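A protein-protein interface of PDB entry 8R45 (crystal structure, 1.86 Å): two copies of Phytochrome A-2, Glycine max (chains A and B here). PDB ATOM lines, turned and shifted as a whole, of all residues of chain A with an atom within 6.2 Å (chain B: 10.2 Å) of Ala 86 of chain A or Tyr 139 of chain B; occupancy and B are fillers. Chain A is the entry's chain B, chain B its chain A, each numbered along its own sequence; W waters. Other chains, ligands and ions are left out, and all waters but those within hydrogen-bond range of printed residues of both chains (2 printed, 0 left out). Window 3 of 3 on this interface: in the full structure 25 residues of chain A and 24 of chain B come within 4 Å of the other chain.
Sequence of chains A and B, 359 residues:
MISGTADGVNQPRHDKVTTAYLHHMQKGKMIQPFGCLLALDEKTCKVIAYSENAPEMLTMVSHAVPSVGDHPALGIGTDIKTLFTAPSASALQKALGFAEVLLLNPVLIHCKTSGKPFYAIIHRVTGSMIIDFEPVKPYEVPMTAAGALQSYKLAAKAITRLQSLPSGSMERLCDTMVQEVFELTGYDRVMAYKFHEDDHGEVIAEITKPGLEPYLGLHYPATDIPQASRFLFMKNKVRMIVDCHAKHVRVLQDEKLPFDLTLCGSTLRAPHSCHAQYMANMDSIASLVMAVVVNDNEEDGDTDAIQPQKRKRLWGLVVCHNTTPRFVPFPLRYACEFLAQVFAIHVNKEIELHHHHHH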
ATOM      1  N   PHE A  84      -9.432 -25.945 -35.147  1.00  0.00           N
ATOM      2  CA  PHE A  84      -9.018 -25.309 -33.905  1.00  0.00           C
ATOM      3  C   PHE A  84      -8.396 -26.333 -32.981  1.00  0.00           C
ATOM      4  O   PHE A  84      -8.711 -27.522 -33.081  1.00  0.00           O
ATOM      5  CB  PHE A  84     -10.228 -24.654 -33.240  1.00  0.00           C
ATOM      6  CG  PHE A  84     -10.979 -23.717 -34.150  1.00  0.00           C
ATOM      7  CD1 PHE A  84     -10.336 -22.678 -34.803  1.00  0.00           C
ATOM      8  CD2 PHE A  84     -12.293 -23.961 -34.469  1.00  0.00           C
ATOM      9  CE1 PHE A  84     -11.054 -21.817 -35.633  1.00  0.00           C
ATOM     10  CE2 PHE A  84     -13.016 -23.118 -35.304  1.00  0.00           C
ATOM     11  CZ  PHE A  84     -12.383 -22.044 -35.907  1.00  0.00           C
ATOM     12  N   THR A  85      -7.599 -25.865 -32.034  1.00  0.00           N
ATOM     13  CA  THR A  85      -7.071 -26.751 -31.015  1.00  0.00           C
ATOM     14  C   THR A  85      -8.219 -27.359 -30.219  1.00  0.00           C
ATOM     15  O   THR A  85      -9.329 -26.833 -30.177  1.00  0.00           O
ATOM     16  CB  THR A  85      -6.147 -26.039 -30.035  1.00  0.00           C
ATOM     17  OG1 THR A  85      -6.888 -25.051 -29.308  1.00  0.00           O
ATOM     18  CG2 THR A  85      -4.946 -25.463 -30.740  1.00  0.00           C
ATOM     19  N   ALA A  86      -7.926 -28.427 -29.488  1.00  0.00           N
ATOM     20  CA  ALA A  86      -9.021 -29.163 -28.867  1.00  0.00           C
ATOM     21  C   ALA A  86      -9.805 -28.320 -27.866  1.00  0.00           C
ATOM     22  O   ALA A  86     -11.055 -28.341 -27.837  1.00  0.00           O
ATOM     23  CB  ALA A  86      -8.506 -30.466 -28.275  1.00  0.00           C
ATOM     24  N   PRO A  87      -9.178 -27.524 -26.983  1.00  0.00           N
ATOM     25  CA  PRO A  87      -9.970 -26.745 -26.050  1.00  0.00           C
ATOM     26  C   PRO A  87     -10.764 -25.660 -26.753  1.00  0.00           C
ATOM     27  O   PRO A  87     -11.851 -25.295 -26.327  1.00  0.00           O
ATOM     28  CB  PRO A  87      -8.961 -26.098 -25.076  1.00  0.00           C
ATOM     29  CG  PRO A  87      -7.703 -26.884 -25.312  1.00  0.00           C
ATOM     30  CD  PRO A  87      -7.745 -27.426 -26.719  1.00  0.00           C
ATOM     31  N   SER A  88     -10.211 -25.130 -27.825  1.00  0.00           N
ATOM     32  CA  SER A  88     -10.906 -24.099 -28.584  1.00  0.00           C
ATOM     33  C   SER A  88     -12.155 -24.690 -29.225  1.00  0.00           C
ATOM     34  O   SER A  88     -13.207 -24.078 -29.179  1.00  0.00           O
ATOM     35  CB  SER A  88     -10.010 -23.500 -29.643  1.00  0.00           C
ATOM     36  OG  SER A  88      -8.954 -22.758 -29.077  1.00  0.00           O
ATOM     37  N   ALA A  89     -12.013 -25.845 -29.894  1.00  0.00           N
ATOM     38  CA  ALA A  89     -13.135 -26.452 -30.603  1.00  0.00           C
ATOM     39  C   ALA A  89     -14.226 -26.861 -29.618  1.00  0.00           C
ATOM     40  O   ALA A  89     -15.412 -26.673 -29.872  1.00  0.00           O
ATOM     41  CB  ALA A  89     -12.659 -27.635 -31.425  1.00  0.00           C
ATOM     42  N   SER A  90     -13.813 -27.359 -28.448  1.00  0.00           N
ATOM     43  CA  SER A  90     -14.754 -27.726 -27.409  1.00  0.00           C
ATOM     44  C   SER A  90     -15.510 -26.515 -26.884  1.00  0.00           C
ATOM     45  O   SER A  90     -16.734 -26.590 -26.667  1.00  0.00           O
ATOM     46  CB  SER A  90     -14.024 -28.481 -26.361  1.00  0.00           C
ATOM     47  OG  SER A  90     -14.870 -28.784 -25.298  1.00  0.00           O
ATOM     48  N   ALA A  91     -14.817 -25.369 -26.690  1.00  0.00           N
ATOM     49  CA  ALA A  91     -15.492 -24.174 -26.220  1.00  0.00           C
ATOM     50  C   ALA A  91     -16.572 -23.743 -27.220  1.00  0.00           C
ATOM     51  O   ALA A  91     -17.646 -23.315 -26.821  1.00  0.00           O
ATOM     52  CB  ALA A  91     -14.533 -23.022 -26.008  1.00  0.00           C
ATOM     53  N   LEU B 108      -2.185 -14.537 -17.991  1.00  0.00           N
ATOM     54  CA  LEU B 108      -2.497 -15.939 -18.173  1.00  0.00           C
ATOM     55  C   LEU B 108      -1.217 -16.603 -18.619  1.00  0.00           C
ATOM     56  O   LEU B 108      -0.705 -16.251 -19.683  1.00  0.00           O
ATOM     57  CB  LEU B 108      -3.626 -16.145 -19.201  1.00  0.00           C
ATOM     58  CG  LEU B 108      -4.132 -17.591 -19.388  1.00  0.00           C
ATOM     59  CD1 LEU B 108      -3.084 -18.576 -19.805  1.00  0.00           C
ATOM     60  CD2 LEU B 108      -4.739 -18.154 -18.135  1.00  0.00           C
ATOM     61  N   HIS B 110       1.152 -20.314 -19.111  1.00  0.00           N
ATOM     62  CA  HIS B 110       1.179 -21.754 -19.338  1.00  0.00           C
ATOM     63  C   HIS B 110       2.566 -22.307 -19.051  1.00  0.00           C
ATOM     64  O   HIS B 110       3.605 -21.738 -19.457  1.00  0.00           O
ATOM     65  CB  HIS B 110       0.862 -22.106 -20.797  1.00  0.00           C
ATOM     66  CG  HIS B 110      -0.498 -21.705 -21.190  1.00  0.00           C
ATOM     67  ND1 HIS B 110      -1.517 -22.634 -21.098  1.00  0.00           N
ATOM     68  CD2 HIS B 110      -1.049 -20.569 -21.620  1.00  0.00           C
ATOM     69  CE1 HIS B 110      -2.650 -22.052 -21.530  1.00  0.00           C
ATOM     70  NE2 HIS B 110      -2.385 -20.788 -21.837  1.00  0.00           N
ATOM     71  N   SER B 114       3.600 -29.226 -20.627  1.00  0.00           N
ATOM     72  CA  SER B 114       2.226 -29.519 -20.166  1.00  0.00           C
ATOM     73  C   SER B 114       1.173 -28.524 -20.658  1.00  0.00           C
ATOM     74  O   SER B 114      -0.002 -28.847 -20.854  1.00  0.00           O
ATOM     75  CB  SER B 114       2.182 -29.581 -18.660  1.00  0.00           C
ATOM     76  OG  SER B 114       2.377 -28.300 -18.066  1.00  0.00           O
ATOM     77  N   GLY B 115       1.583 -27.268 -20.831  1.00  0.00           N
ATOM     78  CA  GLY B 115       0.645 -26.198 -21.086  1.00  0.00           C
ATOM     79  C   GLY B 115      -0.214 -25.906 -19.851  1.00  0.00           C
ATOM     80  O   GLY B 115      -1.201 -25.199 -19.946  1.00  0.00           O
ATOM     81  N   LYS B 116       0.141 -26.437 -18.681  1.00  0.00           N
ATOM     82  CA  LYS B 116      -0.699 -26.247 -17.509  1.00  0.00           C
ATOM     83  C   LYS B 116      -0.879 -24.754 -17.185  1.00  0.00           C
ATOM     84  O   LYS B 116       0.091 -23.998 -17.049  1.00  0.00           O
ATOM     85  CB  LYS B 116      -0.053 -26.974 -16.341  1.00  0.00           C
ATOM     86  CG  LYS B 116      -0.925 -27.147 -15.121  1.00  0.00           C
ATOM     87  CD  LYS B 116      -0.152 -27.741 -13.957  1.00  0.00           C
ATOM     88  CE  LYS B 116      -1.108 -28.066 -12.830  1.00  0.00           C
ATOM     89  NZ  LYS B 116      -0.411 -28.151 -11.540  1.00  0.00           N
ATOM     90  N   PRO B 117      -2.128 -24.266 -17.122  1.00  0.00           N
ATOM     91  CA  PRO B 117      -2.389 -22.838 -17.015  1.00  0.00           C
ATOM     92  C   PRO B 117      -2.628 -22.325 -15.600  1.00  0.00           C
ATOM     93  O   PRO B 117      -3.170 -23.024 -14.756  1.00  0.00           O
ATOM     94  CB  PRO B 117      -3.648 -22.665 -17.882  1.00  0.00           C
ATOM     95  CG  PRO B 117      -4.408 -23.952 -17.647  1.00  0.00           C
ATOM     96  CD  PRO B 117      -3.369 -25.021 -17.397  1.00  0.00           C
ATOM     97  N   PHE B 118      -2.210 -21.084 -15.387  1.00  0.00           N
ATOM     98  CA  PHE B 118      -2.356 -20.337 -14.145  1.00  0.00           C
ATOM     99  C   PHE B 118      -2.653 -18.890 -14.473  1.00  0.00           C
ATOM    100  O   PHE B 118      -2.164 -18.354 -15.473  1.00  0.00           O
ATOM    101  CB  PHE B 118      -1.080 -20.354 -13.308  1.00  0.00           C
ATOM    102  CG  PHE B 118      -0.712 -21.736 -12.830  1.00  0.00           C
ATOM    103  CD1 PHE B 118      -0.064 -22.630 -13.677  1.00  0.00           C
ATOM    104  CD2 PHE B 118      -0.985 -22.122 -11.524  1.00  0.00           C
ATOM    105  CE1 PHE B 118       0.251 -23.898 -13.225  1.00  0.00           C
ATOM    106  CE2 PHE B 118      -0.668 -23.397 -11.076  1.00  0.00           C
ATOM    107  CZ  PHE B 118      -0.036 -24.274 -11.928  1.00  0.00           C
ATOM    108  N   PRO B 135      -4.153 -21.692 -10.081  1.00  0.00           N
ATOM    109  CA  PRO B 135      -4.462 -22.581 -11.188  1.00  0.00           C
ATOM    110  C   PRO B 135      -5.781 -22.253 -11.860  1.00  0.00           C
ATOM    111  O   PRO B 135      -6.717 -21.801 -11.213  1.00  0.00           O
ATOM    112  CB  PRO B 135      -4.542 -23.998 -10.608  1.00  0.00           C
ATOM    113  CG  PRO B 135      -4.319 -23.834  -9.124  1.00  0.00           C
ATOM    114  CD  PRO B 135      -3.979 -22.396  -8.807  1.00  0.00           C
ATOM    115  N   VAL B 136      -5.802 -22.515 -13.164  1.00  0.00           N
ATOM    116  CA  VAL B 136      -6.982 -22.376 -14.011  1.00  0.00           C
ATOM    117  C   VAL B 136      -7.291 -23.728 -14.655  1.00  0.00           C
ATOM    118  O   VAL B 136      -6.399 -24.473 -15.012  1.00  0.00           O
ATOM    119  CB  VAL B 136      -6.774 -21.293 -15.078  1.00  0.00           C
ATOM    120  CG1 VAL B 136      -7.904 -21.306 -16.099  1.00  0.00           C
ATOM    121  CG2 VAL B 136      -6.652 -19.913 -14.431  1.00  0.00           C
ATOM    122  N   LYS B 137      -8.564 -24.044 -14.793  1.00  0.00           N
ATOM    123  CA  LYS B 137      -8.931 -25.320 -15.391  1.00  0.00           C
ATOM    124  C   LYS B 137      -8.607 -25.259 -16.885  1.00  0.00           C
ATOM    125  O   LYS B 137      -9.029 -24.335 -17.562  1.00  0.00           O
ATOM    126  CB  LYS B 137     -10.397 -25.548 -15.093  1.00  0.00           C
ATOM    127  CG  LYS B 137     -10.910 -26.826 -15.684  1.00  0.00           C
ATOM    128  CD  LYS B 137     -12.268 -27.164 -15.242  1.00  0.00           C
ATOM    129  CE  LYS B 137     -12.672 -28.528 -15.766  1.00  0.00           C
ATOM    130  NZ  LYS B 137     -14.112 -28.765 -15.497  1.00  0.00           N
ATOM    131  N   PRO B 138      -7.788 -26.167 -17.455  1.00  0.00           N
ATOM    132  CA  PRO B 138      -7.344 -26.007 -18.837  1.00  0.00           C
ATOM    133  C   PRO B 138      -8.449 -25.780 -19.860  1.00  0.00           C
ATOM    134  O   PRO B 138      -8.300 -24.906 -20.718  1.00  0.00           O
ATOM    135  CB  PRO B 138      -6.588 -27.301 -19.149  1.00  0.00           C
ATOM    136  CG  PRO B 138      -6.136 -27.816 -17.787  1.00  0.00           C
ATOM    137  CD  PRO B 138      -7.153 -27.322 -16.782  1.00  0.00           C
ATOM    138  N   TYR B 139      -9.572 -26.487 -19.745  1.00  0.00           N
ATOM    139  CA  TYR B 139     -10.608 -26.318 -20.768  1.00  0.00           C
ATOM    140  C   TYR B 139     -11.357 -24.988 -20.557  1.00  0.00           C
ATOM    141  O   TYR B 139     -12.158 -24.606 -21.395  1.00  0.00           O
ATOM    142  CB  TYR B 139     -11.559 -27.521 -20.894  1.00  0.00           C
ATOM    143  CG  TYR B 139     -11.072 -28.526 -21.927  1.00  0.00           C
ATOM    144  CD1 TYR B 139      -9.920 -29.280 -21.747  1.00  0.00           C
ATOM    145  CD2 TYR B 139     -11.761 -28.710 -23.113  1.00  0.00           C
ATOM    146  CE1 TYR B 139      -9.454 -30.174 -22.714  1.00  0.00           C
ATOM    147  CE2 TYR B 139     -11.331 -29.618 -24.070  1.00  0.00           C
ATOM    148  CZ  TYR B 139     -10.163 -30.328 -23.895  1.00  0.00           C
ATOM    149  OH  TYR B 139      -9.836 -31.137 -24.923  1.00  0.00           O
ATOM    150  N   GLU B 140     -11.101 -24.265 -19.462  1.00  0.00           N
ATOM    151  CA  GLU B 140     -11.684 -22.937 -19.282  1.00  0.00           C
ATOM    152  C   GLU B 140     -10.800 -21.816 -19.852  1.00  0.00           C
ATOM    153  O   GLU B 140     -11.242 -20.655 -19.885  1.00  0.00           O
ATOM    154  CB  GLU B 140     -11.977 -22.647 -17.811  1.00  0.00           C
ATOM    155  CG  GLU B 140     -13.117 -23.535 -17.286  1.00  0.00           C
ATOM    156  CD  GLU B 140     -13.468 -23.362 -15.814  1.00  0.00           C
ATOM    157  OE1 GLU B 140     -12.799 -22.545 -15.112  1.00  0.00           O
ATOM    158  OE2 GLU B 140     -14.426 -24.052 -15.379  1.00  0.00           O
ATOM    159  N   VAL B 141      -9.577 -22.134 -20.259  1.00  0.00           N
ATOM    160  CA  VAL B 141      -8.672 -21.117 -20.776  1.00  0.00           C
ATOM    161  C   VAL B 141      -9.334 -20.315 -21.909  1.00  0.00           C
ATOM    162  O   VAL B 141      -9.209 -19.089 -21.932  1.00  0.00           O
ATOM    163  CB  VAL B 141      -7.314 -21.720 -21.183  1.00  0.00           C
ATOM    164  CG1 VAL B 141      -6.469 -20.803 -22.070  1.00  0.00           C
ATOM    165  CG2 VAL B 141      -6.503 -22.095 -19.940  1.00  0.00           C
ATOM    166  N   PRO B 142     -10.036 -20.893 -22.895  1.00  0.00           N
ATOM    167  CA  PRO B 142     -10.671 -20.064 -23.924  1.00  0.00           C
ATOM    168  C   PRO B 142     -11.676 -19.033 -23.400  1.00  0.00           C
ATOM    169  O   PRO B 142     -11.981 -18.088 -24.128  1.00  0.00           O
ATOM    170  CB  PRO B 142     -11.386 -21.099 -24.832  1.00  0.00           C
ATOM    171  CG  PRO B 142     -10.549 -22.372 -24.638  1.00  0.00           C
ATOM    172  CD  PRO B 142     -10.257 -22.343 -23.156  1.00  0.00           C
ATOM    173  N   MET B 143     -12.217 -19.243 -22.191  1.00  0.00           N
ATOM    174  CA  MET B 143     -13.236 -18.371 -21.648  1.00  0.00           C
ATOM    175  C   MET B 143     -12.654 -17.357 -20.660  1.00  0.00           C
ATOM    176  O   MET B 143     -13.403 -16.699 -19.945  1.00  0.00           O
ATOM    177  CB  MET B 143     -14.343 -19.164 -20.933  1.00  0.00           C
ATOM    178  CG  MET B 143     -15.003 -20.184 -21.821  1.00  0.00           C
ATOM    179  SD  MET B 143     -15.621 -19.506 -23.383  1.00  0.00           S
ATOM    180  CE  MET B 143     -16.915 -18.428 -22.798  1.00  0.00           C
ATOM    181  N   THR B 144     -11.317 -17.185 -20.596  1.00  0.00           N
ATOM    182  CA  THR B 144     -10.766 -16.301 -19.563  1.00  0.00           C
ATOM    183  C   THR B 144     -11.218 -14.851 -19.733  1.00  0.00           C
ATOM    184  O   THR B 144     -11.617 -14.255 -18.735  1.00  0.00           O
ATOM    185  CB  THR B 144      -9.230 -16.376 -19.418  1.00  0.00           C
ATOM    186  OG1 THR B 144      -8.651 -16.110 -20.674  1.00  0.00           O
ATOM    187  CG2 THR B 144      -8.714 -17.743 -19.083  1.00  0.00           C
HETATM  188  O   HOH W   1     -13.090 -25.499 -23.690  1.00  0.00           O
HETATM  189  O   HOH W   2     -18.188 -21.660 -24.652  1.00  0.00           O
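Water W1 lies within hydrogen-bond range of O of Tyr 139 of chain B, O of Pro 87 of chain A and N of Ala 91 of chain A. Water W2 lies within hydrogen-bond range of the backbone carbonyl oxygen (O) of Ala 91 of chain A (2.8 Å) and the side-chain sulfur (SD) of Met 143 of chain B (3.6 Å).
Printed residues of chain B that touch a printed residue of chain A: Tyr 139 and Pro 142. Hydrophobic or aromatic side chains of chain B that line the printed part of chain A: Tyr 139 and Pro 142. Of the 8 printed residues of chain A, 4 touch a printed residue of chain B. Printed residues of chain A that touch a printed residue of chain B: Ala 86, Pro 87, Ser 90 and Ala 91. Among the printed residues, no Asp or Glu carboxylate lies within 4 Å of a Lys or Arg side-chain nitrogen of the other chain.
Among the printed residues, merely in contact across the chains: Pro 87 of chain A with Pro 142 of chain B, Ala 86 of chain A with Tyr 139 of chain B, Ser 90 of chain A with Tyr 139 of chain B, Pro 87 of chain A with Tyr 139 of chain B and Ala 91 of chain A with Pro 142 of chain B.
Of chain B, only Tyr 139 (3.7 Å) comes within 4 Å of Ala 86 of chain A. No residue of chain B comes within 4 Å of Ser 88 of chain A. Ser 90 of chain A touches one residue of chain B. Of the printed residues of chain B, Ala 91 of chain A touches Pro 142 (3.9 Å). Of the printed residues of chain A, Tyr 139 of chain B touches Ala 86 (3.7 Å), Pro 87 (3.7 Å) and Ser 90 (3.7 Å). Glu 140 of chain B touches none of the printed residues of chain A. Printed residues of chain A within 4 Å of Pro 142 of chain B: Pro 87 and Ala 91. The nearest residue of chain A that does not touch Tyr 139 of chain B is Ala 91 of chain A (5.4 Å). The nearest printed residue of chain B that does not touch Ala 91 of chain A is Met 143 of chain B (4.5 Å).
No position is printed for both chains. Of the 5 pairs that touch across the chains among the printed residues, none has its exchanged pair printed and touching as well.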
